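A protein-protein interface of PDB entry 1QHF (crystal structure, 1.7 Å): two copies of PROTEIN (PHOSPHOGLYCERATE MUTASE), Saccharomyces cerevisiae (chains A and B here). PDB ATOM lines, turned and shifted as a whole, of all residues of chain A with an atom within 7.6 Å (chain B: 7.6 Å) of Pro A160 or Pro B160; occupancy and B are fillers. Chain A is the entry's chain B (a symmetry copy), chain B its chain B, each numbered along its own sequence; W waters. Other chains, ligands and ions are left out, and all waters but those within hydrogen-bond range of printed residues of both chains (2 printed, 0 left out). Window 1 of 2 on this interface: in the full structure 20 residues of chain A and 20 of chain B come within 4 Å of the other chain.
OD1 of Asp A164 sits at hydrogen-bond distance from NE1 of Trp B82.
The guanidinium group of Arg B83 is in salt-bridge range of the side-chain carboxylate of Asp A164 (2.8 Å).
The guanidinium group (NH2) of Arg A83 lies within hydrogen-bond range of the side-chain amide oxygen (OE1) of Gln B163 (2.9 Å).
The guanidinium group (NH2) of Arg B83 lies within hydrogen-bond range of the side-chain amide oxygen (OE1) of Gln A163 (2.9 Å).
OD1 of Asp B164 is in hydrogen-bond range of NE1 of Trp A82.
OD2 of Asp B164 is in salt-bridge range of NE of Arg A83 (2.8 Å).
O of Arg A83 lies within hydrogen-bond range of NH1 of Arg A157 (2.8 Å).
The guanidinium group (NH1) of Arg B157 lies within hydrogen-bond range of the backbone carbonyl oxygen (O) of Arg B83 (2.8 Å).
Pro B160 touches Arg A83 (O to NH2, 3.7 Å).
CD of Gln B163 touches CG2 of Val A144, at 3.4 Å.
Arg B83 touches Pro A160.
Pro B160 touches Pro A160 (CB to CB, 3.5 Å).
Val B144 touches Gln A163.
Of chain B, only Arg B83 and Pro B160 come within 4 Å of Pro A160.
Printed residues of chain A within 4 Å of Trp B82: Asp A164 (3.0 Å).
Printed residues of chain A within 4 Å of Asp B164: Trp A82 and Arg A83.
Of the printed residues of chain B, Gln A163 touches Arg B83 (2.9 Å) and Val B144 (3.4 Å).
The nearest residue of chain A that does not touch Pro B160 is Asp A156 (5.9 Å).
The nearest printed residue of chain A that does not touch Val B144 is Asp A164 (5.2 Å).
Hydrophobic or aromatic side chains of chain B that line the printed part of chain A: Trp B82, Val B144 and Pro B160.
Among the printed residues, 11 pairs touch across the chains.
Among the printed residues, Asp or Glu carboxylates within 4 Å of a Lys or Arg side-chain nitrogen of the other chain: Arg A83 with Asp B164 (2.8 Å) and Asp A164 with Arg B83 (2.8 Å).
Arg A83 touches Gln B163, and with the chains exchanged Gln A163 touches Arg B83.
Arg A83 touches Asp B164, and with the chains exchanged Asp A164 touches Arg B83.
Val A144 touches Gln B163, and with the chains exchanged Gln A163 touches Val B144.
Pro B160 touches its own counterpart, Pro A160.
Positions printed for both chains: 82, 83, 144, 154, 155, 156, 157, 158, 159, 160, 161, 162, 163, 164, 165, 166 and 167.
Of the 11 pairs that touch across the chains among the printed residues, 11 have their exchanged pair printed and touching as well.
Water W1 bridges NH1 of Arg A83 (2.8 Å) and OE1 of Gln B163 (2.8 Å).
Water W2 lies within hydrogen-bond range of NH1 of Arg B83 and OE1 of Gln A163.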
ATOM      1  N   TRP A  82       2.485  -1.622  -0.098  1.00  0.00           N
ATOM      2  CA  TRP A  82       2.811  -0.292   0.427  1.00  0.00           C
ATOM      3  C   TRP A  82       1.530   0.387   0.888  1.00  0.00           C
ATOM      4  O   TRP A  82       1.514   1.319   1.706  1.00  0.00           O
ATOM      5  CB  TRP A  82       3.447   0.533  -0.701  1.00  0.00           C
ATOM      6  CG  TRP A  82       2.551   1.068  -1.764  1.00  0.00           C
ATOM      7  CD1 TRP A  82       2.254   0.486  -2.959  1.00  0.00           C
ATOM      8  CD2 TRP A  82       1.880   2.333  -1.761  1.00  0.00           C
ATOM      9  NE1 TRP A  82       1.389   1.272  -3.692  1.00  0.00           N
ATOM     10  CE2 TRP A  82       1.167   2.426  -2.980  1.00  0.00           C
ATOM     11  CE3 TRP A  82       1.769   3.385  -0.856  1.00  0.00           C
ATOM     12  CZ2 TRP A  82       0.376   3.537  -3.298  1.00  0.00           C
ATOM     13  CZ3 TRP A  82       1.024   4.510  -1.180  1.00  0.00           C
ATOM     14  CH2 TRP A  82       0.323   4.586  -2.408  1.00  0.00           C
ATOM     15  N   ARG A  83       0.351   0.000   0.349  1.00  0.00           N
ATOM     16  CA  ARG A  83      -0.906   0.663   0.711  1.00  0.00           C
ATOM     17  C   ARG A  83      -1.312   0.417   2.170  1.00  0.00           C
ATOM     18  O   ARG A  83      -2.227   1.110   2.623  1.00  0.00           O
ATOM     19  CB  ARG A  83      -2.016   0.236  -0.265  1.00  0.00           C
ATOM     20  CG  ARG A  83      -1.709   0.805  -1.672  1.00  0.00           C
ATOM     21  CD  ARG A  83      -2.787   0.369  -2.676  1.00  0.00           C
ATOM     22  NE  ARG A  83      -2.367   0.938  -3.978  1.00  0.00           N
ATOM     23  CZ  ARG A  83      -2.708   2.108  -4.497  1.00  0.00           C
ATOM     24  NH1 ARG A  83      -3.550   2.938  -3.898  1.00  0.00           N
ATOM     25  NH2 ARG A  83      -2.159   2.399  -5.708  1.00  0.00           N
ATOM     26  N   VAL A 144       3.006   8.050  -7.520  1.00  0.00           N
ATOM     27  CA  VAL A 144       2.010   7.946  -6.465  1.00  0.00           C
ATOM     28  C   VAL A 144       2.673   7.897  -5.092  1.00  0.00           C
ATOM     29  O   VAL A 144       1.965   8.147  -4.134  1.00  0.00           O
ATOM     30  CB  VAL A 144       1.086   6.732  -6.718  1.00  0.00           C
ATOM     31  CG1 VAL A 144       1.773   5.414  -6.450  1.00  0.00           C
ATOM     32  CG2 VAL A 144      -0.222   6.839  -5.961  1.00  0.00           C
ATOM     33  N   VAL A 154      -4.104   8.802   3.551  1.00  0.00           N
ATOM     34  CA  VAL A 154      -3.854   7.366   3.810  1.00  0.00           C
ATOM     35  C   VAL A 154      -5.069   6.551   3.392  1.00  0.00           C
ATOM     36  O   VAL A 154      -4.990   5.513   2.729  1.00  0.00           O
ATOM     37  CB  VAL A 154      -3.573   7.099   5.312  1.00  0.00           C
ATOM     38  CG1 VAL A 154      -3.616   5.621   5.698  1.00  0.00           C
ATOM     39  CG2 VAL A 154      -2.228   7.707   5.661  1.00  0.00           C
ATOM     40  N   ILE A 155      -6.268   6.991   3.796  1.00  0.00           N
ATOM     41  CA  ILE A 155      -7.476   6.237   3.461  1.00  0.00           C
ATOM     42  C   ILE A 155      -7.664   6.158   1.948  1.00  0.00           C
ATOM     43  O   ILE A 155      -7.993   5.068   1.445  1.00  0.00           O
ATOM     44  CB  ILE A 155      -8.708   6.899   4.101  1.00  0.00           C
ATOM     45  CG1 ILE A 155      -8.705   6.619   5.624  1.00  0.00           C
ATOM     46  CG2 ILE A 155     -10.001   6.325   3.508  1.00  0.00           C
ATOM     47  CD1 ILE A 155      -9.700   7.495   6.387  1.00  0.00           C
ATOM     48  N   ASP A 156      -7.366   7.231   1.243  1.00  0.00           N
ATOM     49  CA  ASP A 156      -7.573   7.206  -0.212  1.00  0.00           C
ATOM     50  C   ASP A 156      -6.659   6.189  -0.894  1.00  0.00           C
ATOM     51  O   ASP A 156      -7.104   5.565  -1.878  1.00  0.00           O
ATOM     52  CB  ASP A 156      -7.398   8.562  -0.870  1.00  0.00           C
ATOM     53  CG  ASP A 156      -8.506   9.549  -0.565  1.00  0.00           C
ATOM     54  OD1 ASP A 156      -9.651   9.189  -0.207  1.00  0.00           O
ATOM     55  OD2 ASP A 156      -8.172  10.746  -0.690  1.00  0.00           O
ATOM     56  N   ARG A 157      -5.383   6.077  -0.479  1.00  0.00           N
ATOM     57  CA  ARG A 157      -4.551   5.020  -1.049  1.00  0.00           C
ATOM     58  C   ARG A 157      -4.742   3.634  -0.465  1.00  0.00           C
ATOM     59  O   ARG A 157      -4.305   2.657  -1.107  1.00  0.00           O
ATOM     60  CB  ARG A 157      -3.066   5.393  -1.176  1.00  0.00           C
ATOM     61  CG  ARG A 157      -2.435   5.945   0.125  1.00  0.00           C
ATOM     62  CD  ARG A 157      -1.991   4.821   1.068  1.00  0.00           C
ATOM     63  NE  ARG A 157      -1.021   5.363   2.036  1.00  0.00           N
ATOM     64  CZ  ARG A 157      -0.594   4.699   3.112  1.00  0.00           C
ATOM     65  NH1 ARG A 157      -1.011   3.493   3.475  1.00  0.00           N
ATOM     66  NH2 ARG A 157       0.273   5.344   3.919  1.00  0.00           N
ATOM     67  N   LEU A 158      -5.354   3.430   0.694  1.00  0.00           N
ATOM     68  CA  LEU A 158      -5.548   2.100   1.265  1.00  0.00           C
ATOM     69  C   LEU A 158      -6.748   1.386   0.668  1.00  0.00           C
ATOM     70  O   LEU A 158      -6.789   0.186   0.410  1.00  0.00           O
ATOM     71  CB  LEU A 158      -5.714   2.247   2.807  1.00  0.00           C
ATOM     72  CG  LEU A 158      -5.816   0.916   3.577  1.00  0.00           C
ATOM     73  CD1 LEU A 158      -5.125   1.127   4.929  1.00  0.00           C
ATOM     74  CD2 LEU A 158      -7.287   0.614   3.803  1.00  0.00           C
ATOM     75  N   LEU A 159      -7.827   2.156   0.462  1.00  0.00           N
ATOM     76  CA  LEU A 159      -9.110   1.535   0.082  1.00  0.00           C
ATOM     77  C   LEU A 159      -9.117   0.690  -1.166  1.00  0.00           C
ATOM     78  O   LEU A 159      -9.673  -0.413  -1.142  1.00  0.00           O
ATOM     79  CB  LEU A 159     -10.197   2.612   0.057  1.00  0.00           C
ATOM     80  CG  LEU A 159     -10.794   3.087   1.380  1.00  0.00           C
ATOM     81  CD1 LEU A 159     -11.988   3.984   1.033  1.00  0.00           C
ATOM     82  CD2 LEU A 159     -11.178   1.939   2.297  1.00  0.00           C
ATOM     83  N   PRO A 160      -8.407   1.019  -2.261  1.00  0.00           N
ATOM     84  CA  PRO A 160      -8.417   0.205  -3.465  1.00  0.00           C
ATOM     85  C   PRO A 160      -7.804  -1.183  -3.209  1.00  0.00           C
ATOM     86  O   PRO A 160      -8.272  -2.164  -3.788  1.00  0.00           O
ATOM     87  CB  PRO A 160      -7.553   0.956  -4.462  1.00  0.00           C
ATOM     88  CG  PRO A 160      -7.650   2.386  -4.016  1.00  0.00           C
ATOM     89  CD  PRO A 160      -7.756   2.333  -2.499  1.00  0.00           C
ATOM     90  N   TYR A 161      -6.838  -1.254  -2.289  1.00  0.00           N
ATOM     91  CA  TYR A 161      -6.269  -2.572  -1.928  1.00  0.00           C
ATOM     92  C   TYR A 161      -7.268  -3.436  -1.168  1.00  0.00           C
ATOM     93  O   TYR A 161      -7.438  -4.661  -1.353  1.00  0.00           O
ATOM     94  CB  TYR A 161      -4.975  -2.368  -1.158  1.00  0.00           C
ATOM     95  CG  TYR A 161      -4.135  -3.626  -1.003  1.00  0.00           C
ATOM     96  CD1 TYR A 161      -3.474  -4.196  -2.092  1.00  0.00           C
ATOM     97  CD2 TYR A 161      -3.972  -4.212   0.240  1.00  0.00           C
ATOM     98  CE1 TYR A 161      -2.709  -5.333  -1.974  1.00  0.00           C
ATOM     99  CE2 TYR A 161      -3.201  -5.360   0.373  1.00  0.00           C
ATOM    100  CZ  TYR A 161      -2.577  -5.907  -0.693  1.00  0.00           C
ATOM    101  OH  TYR A 161      -1.775  -7.019  -0.617  1.00  0.00           O
ATOM    102  N   TRP A 162      -7.956  -2.813  -0.217  1.00  0.00           N
ATOM    103  CA  TRP A 162      -9.015  -3.401   0.558  1.00  0.00           C
ATOM    104  C   TRP A 162     -10.106  -3.851  -0.416  1.00  0.00           C
ATOM    105  O   TRP A 162     -10.563  -5.006  -0.328  1.00  0.00           O
ATOM    106  CB  TRP A 162      -9.578  -2.328   1.530  1.00  0.00           C
ATOM    107  CG  TRP A 162     -10.926  -2.756   2.052  1.00  0.00           C
ATOM    108  CD1 TRP A 162     -12.136  -2.283   1.624  1.00  0.00           C
ATOM    109  CD2 TRP A 162     -11.206  -3.749   3.051  1.00  0.00           C
ATOM    110  NE1 TRP A 162     -13.134  -2.932   2.301  1.00  0.00           N
ATOM    111  CE2 TRP A 162     -12.600  -3.829   3.178  1.00  0.00           C
ATOM    112  CE3 TRP A 162     -10.401  -4.562   3.850  1.00  0.00           C
ATOM    113  CZ2 TRP A 162     -13.235  -4.691   4.074  1.00  0.00           C
ATOM    114  CZ3 TRP A 162     -11.027  -5.432   4.750  1.00  0.00           C
ATOM    115  CH2 TRP A 162     -12.431  -5.483   4.846  1.00  0.00           C
ATOM    116  N   GLN A 163     -10.471  -2.995  -1.379  1.00  0.00           N
ATOM    117  CA  GLN A 163     -11.617  -3.365  -2.231  1.00  0.00           C
ATOM    118  C   GLN A 163     -11.424  -4.513  -3.156  1.00  0.00           C
ATOM    119  O   GLN A 163     -12.349  -5.304  -3.414  1.00  0.00           O
ATOM    120  CB  GLN A 163     -11.960  -2.118  -3.107  1.00  0.00           C
ATOM    121  CG  GLN A 163     -12.539  -0.995  -2.256  1.00  0.00           C
ATOM    122  CD  GLN A 163     -12.402   0.373  -2.890  1.00  0.00           C
ATOM    123  OE1 GLN A 163     -11.763   0.594  -3.910  1.00  0.00           O
ATOM    124  NE2 GLN A 163     -13.040   1.367  -2.229  1.00  0.00           N
ATOM    125  N   ASP A 164     -10.226  -4.660  -3.752  1.00  0.00           N
ATOM    126  CA  ASP A 164      -9.998  -5.720  -4.727  1.00  0.00           C
ATOM    127  C   ASP A 164      -9.248  -6.947  -4.192  1.00  0.00           C
ATOM    128  O   ASP A 164      -9.434  -8.028  -4.751  1.00  0.00           O
ATOM    129  CB  ASP A 164      -9.154  -5.187  -5.891  1.00  0.00           C
ATOM    130  CG  ASP A 164      -9.891  -4.215  -6.801  1.00  0.00           C
ATOM    131  OD1 ASP A 164     -11.031  -3.845  -6.501  1.00  0.00           O
ATOM    132  OD2 ASP A 164      -9.255  -3.906  -7.833  1.00  0.00           O
ATOM    133  N   VAL A 165      -8.327  -6.688  -3.236  1.00  0.00           N
ATOM    134  CA  VAL A 165      -7.448  -7.817  -2.869  1.00  0.00           C
ATOM    135  C   VAL A 165      -7.851  -8.414  -1.527  1.00  0.00           C
ATOM    136  O   VAL A 165      -8.170  -9.627  -1.493  1.00  0.00           O
ATOM    137  CB  VAL A 165      -6.005  -7.252  -2.789  1.00  0.00           C
ATOM    138  CG1 VAL A 165      -5.008  -8.314  -2.359  1.00  0.00           C
ATOM    139  CG2 VAL A 165      -5.587  -6.601  -4.101  1.00  0.00           C
ATOM    140  N   ILE A 166      -7.923  -7.574  -0.497  1.00  0.00           N
ATOM    141  CA  ILE A 166      -8.294  -8.203   0.804  1.00  0.00           C
ATOM    142  C   ILE A 166      -9.742  -8.673   0.736  1.00  0.00           C
ATOM    143  O   ILE A 166     -10.066  -9.764   1.203  1.00  0.00           O
ATOM    144  CB  ILE A 166      -8.098  -7.131   1.896  1.00  0.00           C
ATOM    145  CG1 ILE A 166      -6.618  -6.761   1.921  1.00  0.00           C
ATOM    146  CG2 ILE A 166      -8.517  -7.713   3.270  1.00  0.00           C
ATOM    147  CD1 ILE A 166      -6.259  -5.639   2.885  1.00  0.00           C
ATOM    148  N   ALA A 167     -10.634  -7.898   0.128  1.00  0.00           N
ATOM    149  CA  ALA A 167     -12.039  -8.312   0.033  1.00  0.00           C
ATOM    150  C   ALA A 167     -12.187  -9.646  -0.670  1.00  0.00           C
ATOM    151  O   ALA A 167     -13.052 -10.436  -0.308  1.00  0.00           O
ATOM    152  CB  ALA A 167     -12.826  -7.278  -0.825  1.00  0.00           C
ATOM    153  N   TRP B  82     -12.129  -5.085 -13.264  1.00  0.00           N
ATOM    154  CA  TRP B  82     -13.306  -4.224 -13.421  1.00  0.00           C
ATOM    155  C   TRP B  82     -12.851  -2.775 -13.525  1.00  0.00           C
ATOM    156  O   TRP B  82     -13.543  -1.883 -14.037  1.00  0.00           O
ATOM    157  CB  TRP B  82     -14.199  -4.389 -12.183  1.00  0.00           C
ATOM    158  CG  TRP B  82     -13.766  -3.729 -10.919  1.00  0.00           C
ATOM    159  CD1 TRP B  82     -13.030  -4.279  -9.914  1.00  0.00           C
ATOM    160  CD2 TRP B  82     -14.100  -2.405 -10.488  1.00  0.00           C
ATOM    161  NE1 TRP B  82     -12.823  -3.371  -8.896  1.00  0.00           N
ATOM    162  CE2 TRP B  82     -13.496  -2.217  -9.221  1.00  0.00           C
ATOM    163  CE3 TRP B  82     -14.810  -1.341 -11.038  1.00  0.00           C
ATOM    164  CZ2 TRP B  82     -13.603  -1.013  -8.515  1.00  0.00           C
ATOM    165  CZ3 TRP B  82     -14.960  -0.159 -10.326  1.00  0.00           C
ATOM    166  CH2 TRP B  82     -14.353   0.006  -9.058  1.00  0.00           C
ATOM    167  N   ARG B  83     -11.658  -2.423 -12.992  1.00  0.00           N
ATOM    168  CA  ARG B  83     -11.199  -1.030 -13.009  1.00  0.00           C
ATOM    169  C   ARG B  83     -10.896  -0.518 -14.424  1.00  0.00           C
ATOM    170  O   ARG B  83     -10.722   0.696 -14.556  1.00  0.00           O
ATOM    171  CB  ARG B  83      -9.984  -0.874 -12.078  1.00  0.00           C
ATOM    172  CG  ARG B  83     -10.432  -1.080 -10.611  1.00  0.00           C
ATOM    173  CD  ARG B  83      -9.231  -0.960  -9.660  1.00  0.00           C
ATOM    174  NE  ARG B  83      -9.775  -1.211  -8.305  1.00  0.00           N
ATOM    175  CZ  ARG B  83     -10.234  -0.320  -7.440  1.00  0.00           C
ATOM    176  NH1 ARG B  83     -10.220   0.984  -7.681  1.00  0.00           N
ATOM    177  NH2 ARG B  83     -10.701  -0.823  -6.264  1.00  0.00           N
ATOM    178  N   VAL B 144     -18.066  -0.803  -3.501  1.00  0.00           N
ATOM    179  CA  VAL B 144     -17.373   0.080  -4.425  1.00  0.00           C
ATOM    180  C   VAL B 144     -17.986   0.001  -5.819  1.00  0.00           C
ATOM    181  O   VAL B 144     -17.729   0.914  -6.583  1.00  0.00           O
ATOM    182  CB  VAL B 144     -15.858  -0.229  -4.427  1.00  0.00           C
ATOM    183  CG1 VAL B 144     -15.531  -1.523  -5.134  1.00  0.00           C
ATOM    184  CG2 VAL B 144     -15.038   0.923  -4.974  1.00  0.00           C
ATOM    185  N   VAL B 154     -14.492   7.555 -13.043  1.00  0.00           N
ATOM    186  CA  VAL B 154     -13.762   6.464 -13.726  1.00  0.00           C
ATOM    187  C   VAL B 154     -12.274   6.577 -13.426  1.00  0.00           C
ATOM    188  O   VAL B 154     -11.576   5.613 -13.099  1.00  0.00           O
ATOM    189  CB  VAL B 154     -13.961   6.520 -15.263  1.00  0.00           C
ATOM    190  CG1 VAL B 154     -12.998   5.628 -16.047  1.00  0.00           C
ATOM    191  CG2 VAL B 154     -15.401   6.157 -15.571  1.00  0.00           C
ATOM    192  N   ILE B 155     -11.716   7.788 -13.553  1.00  0.00           N
ATOM    193  CA  ILE B 155     -10.283   7.963 -13.315  1.00  0.00           C
ATOM    194  C   ILE B 155      -9.924   7.600 -11.876  1.00  0.00           C
ATOM    195  O   ILE B 155      -8.905   6.914 -11.671  1.00  0.00           O
ATOM    196  CB  ILE B 155      -9.872   9.418 -13.600  1.00  0.00           C
ATOM    197  CG1 ILE B 155      -9.859   9.654 -15.130  1.00  0.00           C
ATOM    198  CG2 ILE B 155      -8.467   9.700 -13.055  1.00  0.00           C
ATOM    199  CD1 ILE B 155      -9.779  11.137 -15.497  1.00  0.00           C
ATOM    200  N   ASP B 156     -10.774   7.951 -10.932  1.00  0.00           N
ATOM    201  CA  ASP B 156     -10.443   7.655  -9.531  1.00  0.00           C
ATOM    202  C   ASP B 156     -10.378   6.152  -9.272  1.00  0.00           C
ATOM    203  O   ASP B 156      -9.528   5.730  -8.464  1.00  0.00           O
ATOM    204  CB  ASP B 156     -11.394   8.298  -8.537  1.00  0.00           C
ATOM    205  CG  ASP B 156     -11.252   9.802  -8.424  1.00  0.00           C
ATOM    206  OD1 ASP B 156     -10.203  10.407  -8.742  1.00  0.00           O
ATOM    207  OD2 ASP B 156     -12.275  10.380  -8.002  1.00  0.00           O
ATOM    208  N   ARG B 157     -11.300   5.351  -9.840  1.00  0.00           N
ATOM    209  CA  ARG B 157     -11.161   3.904  -9.690  1.00  0.00           C
ATOM    210  C   ARG B 157     -10.171   3.231 -10.620  1.00  0.00           C
ATOM    211  O   ARG B 157      -9.781   2.080 -10.335  1.00  0.00           O
ATOM    212  CB  ARG B 157     -12.498   3.150  -9.627  1.00  0.00           C
ATOM    213  CG  ARG B 157     -13.474   3.490 -10.778  1.00  0.00           C
ATOM    214  CD  ARG B 157     -13.169   2.683 -12.045  1.00  0.00           C
ATOM    215  NE  ARG B 157     -14.355   2.697 -12.920  1.00  0.00           N
ATOM    216  CZ  ARG B 157     -14.355   2.260 -14.181  1.00  0.00           C
ATOM    217  NH1 ARG B 157     -13.290   1.797 -14.824  1.00  0.00           N
ATOM    218  NH2 ARG B 157     -15.514   2.368 -14.861  1.00  0.00           N
ATOM    219  N   LEU B 158      -9.708   3.822 -11.713  1.00  0.00           N
ATOM    220  CA  LEU B 158      -8.751   3.186 -12.614  1.00  0.00           C
ATOM    221  C   LEU B 158      -7.322   3.309 -12.117  1.00  0.00           C
ATOM    222  O   LEU B 158      -6.473   2.427 -12.209  1.00  0.00           O
ATOM    223  CB  LEU B 158      -8.895   3.837 -14.023  1.00  0.00           C
ATOM    224  CG  LEU B 158      -8.027   3.195 -15.124  1.00  0.00           C
ATOM    225  CD1 LEU B 158      -8.830   3.272 -16.427  1.00  0.00           C
ATOM    226  CD2 LEU B 158      -6.759   4.018 -15.262  1.00  0.00           C
ATOM    227  N   LEU B 159      -7.003   4.497 -11.582  1.00  0.00           N
ATOM    228  CA  LEU B 159      -5.597   4.801 -11.255  1.00  0.00           C
ATOM    229  C   LEU B 159      -4.897   3.861 -10.307  1.00  0.00           C
ATOM    230  O   LEU B 159      -3.760   3.466 -10.583  1.00  0.00           O
ATOM    231  CB  LEU B 159      -5.494   6.260 -10.805  1.00  0.00           C
ATOM    232  CG  LEU B 159      -5.509   7.361 -11.863  1.00  0.00           C
ATOM    233  CD1 LEU B 159      -5.172   8.673 -11.146  1.00  0.00           C
ATOM    234  CD2 LEU B 159      -4.569   7.075 -13.021  1.00  0.00           C
ATOM    235  N   PRO B 160      -5.522   3.311  -9.249  1.00  0.00           N
ATOM    236  CA  PRO B 160      -4.845   2.408  -8.333  1.00  0.00           C
ATOM    237  C   PRO B 160      -4.416   1.111  -9.039  1.00  0.00           C
ATOM    238  O   PRO B 160      -3.357   0.570  -8.716  1.00  0.00           O
ATOM    239  CB  PRO B 160      -5.873   2.079  -7.265  1.00  0.00           C
ATOM    240  CG  PRO B 160      -6.791   3.265  -7.273  1.00  0.00           C
ATOM    241  CD  PRO B 160      -6.845   3.730  -8.720  1.00  0.00           C
ATOM    242  N   TYR B 161      -5.190   0.687 -10.043  1.00  0.00           N
ATOM    243  CA  TYR B 161      -4.786  -0.503 -10.825  1.00  0.00           C
ATOM    244  C   TYR B 161      -3.556  -0.230 -11.684  1.00  0.00           C
ATOM    245  O   TYR B 161      -2.603  -1.025 -11.837  1.00  0.00           O
ATOM    246  CB  TYR B 161      -5.968  -0.994 -11.643  1.00  0.00           C
ATOM    247  CG  TYR B 161      -5.782  -2.380 -12.241  1.00  0.00           C
ATOM    248  CD1 TYR B 161      -5.779  -3.521 -11.440  1.00  0.00           C
ATOM    249  CD2 TYR B 161      -5.654  -2.541 -13.610  1.00  0.00           C
ATOM    250  CE1 TYR B 161      -5.612  -4.784 -11.960  1.00  0.00           C
ATOM    251  CE2 TYR B 161      -5.488  -3.811 -14.149  1.00  0.00           C
ATOM    252  CZ  TYR B 161      -5.473  -4.906 -13.358  1.00  0.00           C
ATOM    253  OH  TYR B 161      -5.348  -6.187 -13.836  1.00  0.00           O
ATOM    254  N   TRP B 162      -3.560   0.927 -12.336  1.00  0.00           N
ATOM    255  CA  TRP B 162      -2.470   1.435 -13.124  1.00  0.00           C
ATOM    256  C   TRP B 162      -1.253   1.563 -12.204  1.00  0.00           C
ATOM    257  O   TRP B 162      -0.162   1.084 -12.567  1.00  0.00           O
ATOM    258  CB  TRP B 162      -2.865   2.830 -13.683  1.00  0.00           C
ATOM    259  CG  TRP B 162      -1.637   3.568 -14.153  1.00  0.00           C
ATOM    260  CD1 TRP B 162      -1.000   4.572 -13.476  1.00  0.00           C
ATOM    261  CD2 TRP B 162      -0.885   3.345 -15.356  1.00  0.00           C
ATOM    262  NE1 TRP B 162       0.095   4.970 -14.195  1.00  0.00           N
ATOM    263  CE2 TRP B 162       0.191   4.243 -15.346  1.00  0.00           C
ATOM    264  CE3 TRP B 162      -1.037   2.476 -16.437  1.00  0.00           C
ATOM    265  CZ2 TRP B 162       1.132   4.316 -16.374  1.00  0.00           C
ATOM    266  CZ3 TRP B 162      -0.098   2.539 -17.472  1.00  0.00           C
ATOM    267  CH2 TRP B 162       0.970   3.456 -17.422  1.00  0.00           C
ATOM    268  N   GLN B 163      -1.439   2.125 -11.004  1.00  0.00           N
ATOM    269  CA  GLN B 163      -0.248   2.380 -10.171  1.00  0.00           C
ATOM    270  C   GLN B 163       0.466   1.189  -9.638  1.00  0.00           C
ATOM    271  O   GLN B 163       1.705   1.174  -9.516  1.00  0.00           O
ATOM    272  CB  GLN B 163      -0.717   3.225  -8.944  1.00  0.00           C
ATOM    273  CG  GLN B 163      -1.120   4.631  -9.370  1.00  0.00           C
ATOM    274  CD  GLN B 163      -2.052   5.313  -8.392  1.00  0.00           C
ATOM    275  OE1 GLN B 163      -2.561   4.756  -7.429  1.00  0.00           O
ATOM    276  NE2 GLN B 163      -2.305   6.614  -8.668  1.00  0.00           N
ATOM    277  N   ASP B 164      -0.263   0.128  -9.246  1.00  0.00           N
ATOM    278  CA  ASP B 164       0.373  -1.038  -8.644  1.00  0.00           C
ATOM    279  C   ASP B 164       0.564  -2.234  -9.585  1.00  0.00           C
ATOM    280  O   ASP B 164       1.476  -3.023  -9.340  1.00  0.00           O
ATOM    281  CB  ASP B 164      -0.477  -1.553  -7.476  1.00  0.00           C
ATOM    282  CG  ASP B 164      -0.468  -0.650  -6.252  1.00  0.00           C
ATOM    283  OD1 ASP B 164       0.103   0.444  -6.307  1.00  0.00           O
ATOM    284  OD2 ASP B 164      -1.032  -1.147  -5.252  1.00  0.00           O
ATOM    285  N   VAL B 165      -0.398  -2.388 -10.524  1.00  0.00           N
ATOM    286  CA  VAL B 165      -0.350  -3.649 -11.292  1.00  0.00           C
ATOM    287  C   VAL B 165       0.195  -3.417 -12.695  1.00  0.00           C
ATOM    288  O   VAL B 165       1.228  -4.042 -13.037  1.00  0.00           O
ATOM    289  CB  VAL B 165      -1.805  -4.182 -11.367  1.00  0.00           C
ATOM    290  CG1 VAL B 165      -1.895  -5.456 -12.189  1.00  0.00           C
ATOM    291  CG2 VAL B 165      -2.400  -4.378  -9.978  1.00  0.00           C
ATOM    292  N   ILE B 166      -0.418  -2.491 -13.429  1.00  0.00           N
ATOM    293  CA  ILE B 166       0.128  -2.314 -14.806  1.00  0.00           C
ATOM    294  C   ILE B 166       1.524  -1.708 -14.715  1.00  0.00           C
ATOM    295  O   ILE B 166       2.431  -2.122 -15.434  1.00  0.00           O
ATOM    296  CB  ILE B 166      -0.844  -1.386 -15.562  1.00  0.00           C
ATOM    297  CG1 ILE B 166      -2.192  -2.096 -15.644  1.00  0.00           C
ATOM    298  CG2 ILE B 166      -0.301  -1.124 -16.990  1.00  0.00           C
ATOM    299  CD1 ILE B 166      -3.304  -1.276 -16.282  1.00  0.00           C
ATOM    300  N   ALA B 167       1.744  -0.753 -13.816  1.00  0.00           N
ATOM    301  CA  ALA B 167       3.073  -0.144 -13.688  1.00  0.00           C
ATOM    302  C   ALA B 167       4.140  -1.176 -13.383  1.00  0.00           C
ATOM    303  O   ALA B 167       5.264  -1.054 -13.856  1.00  0.00           O
ATOM    304  CB  ALA B 167       3.073   0.850 -12.490  1.00  0.00           C
HETATM  305  O   HOH W   1      -3.838   5.494  -5.021  1.00  0.00           O
HETATM  306  O   HOH W   2     -11.565   2.634  -5.852  1.00  0.00           O
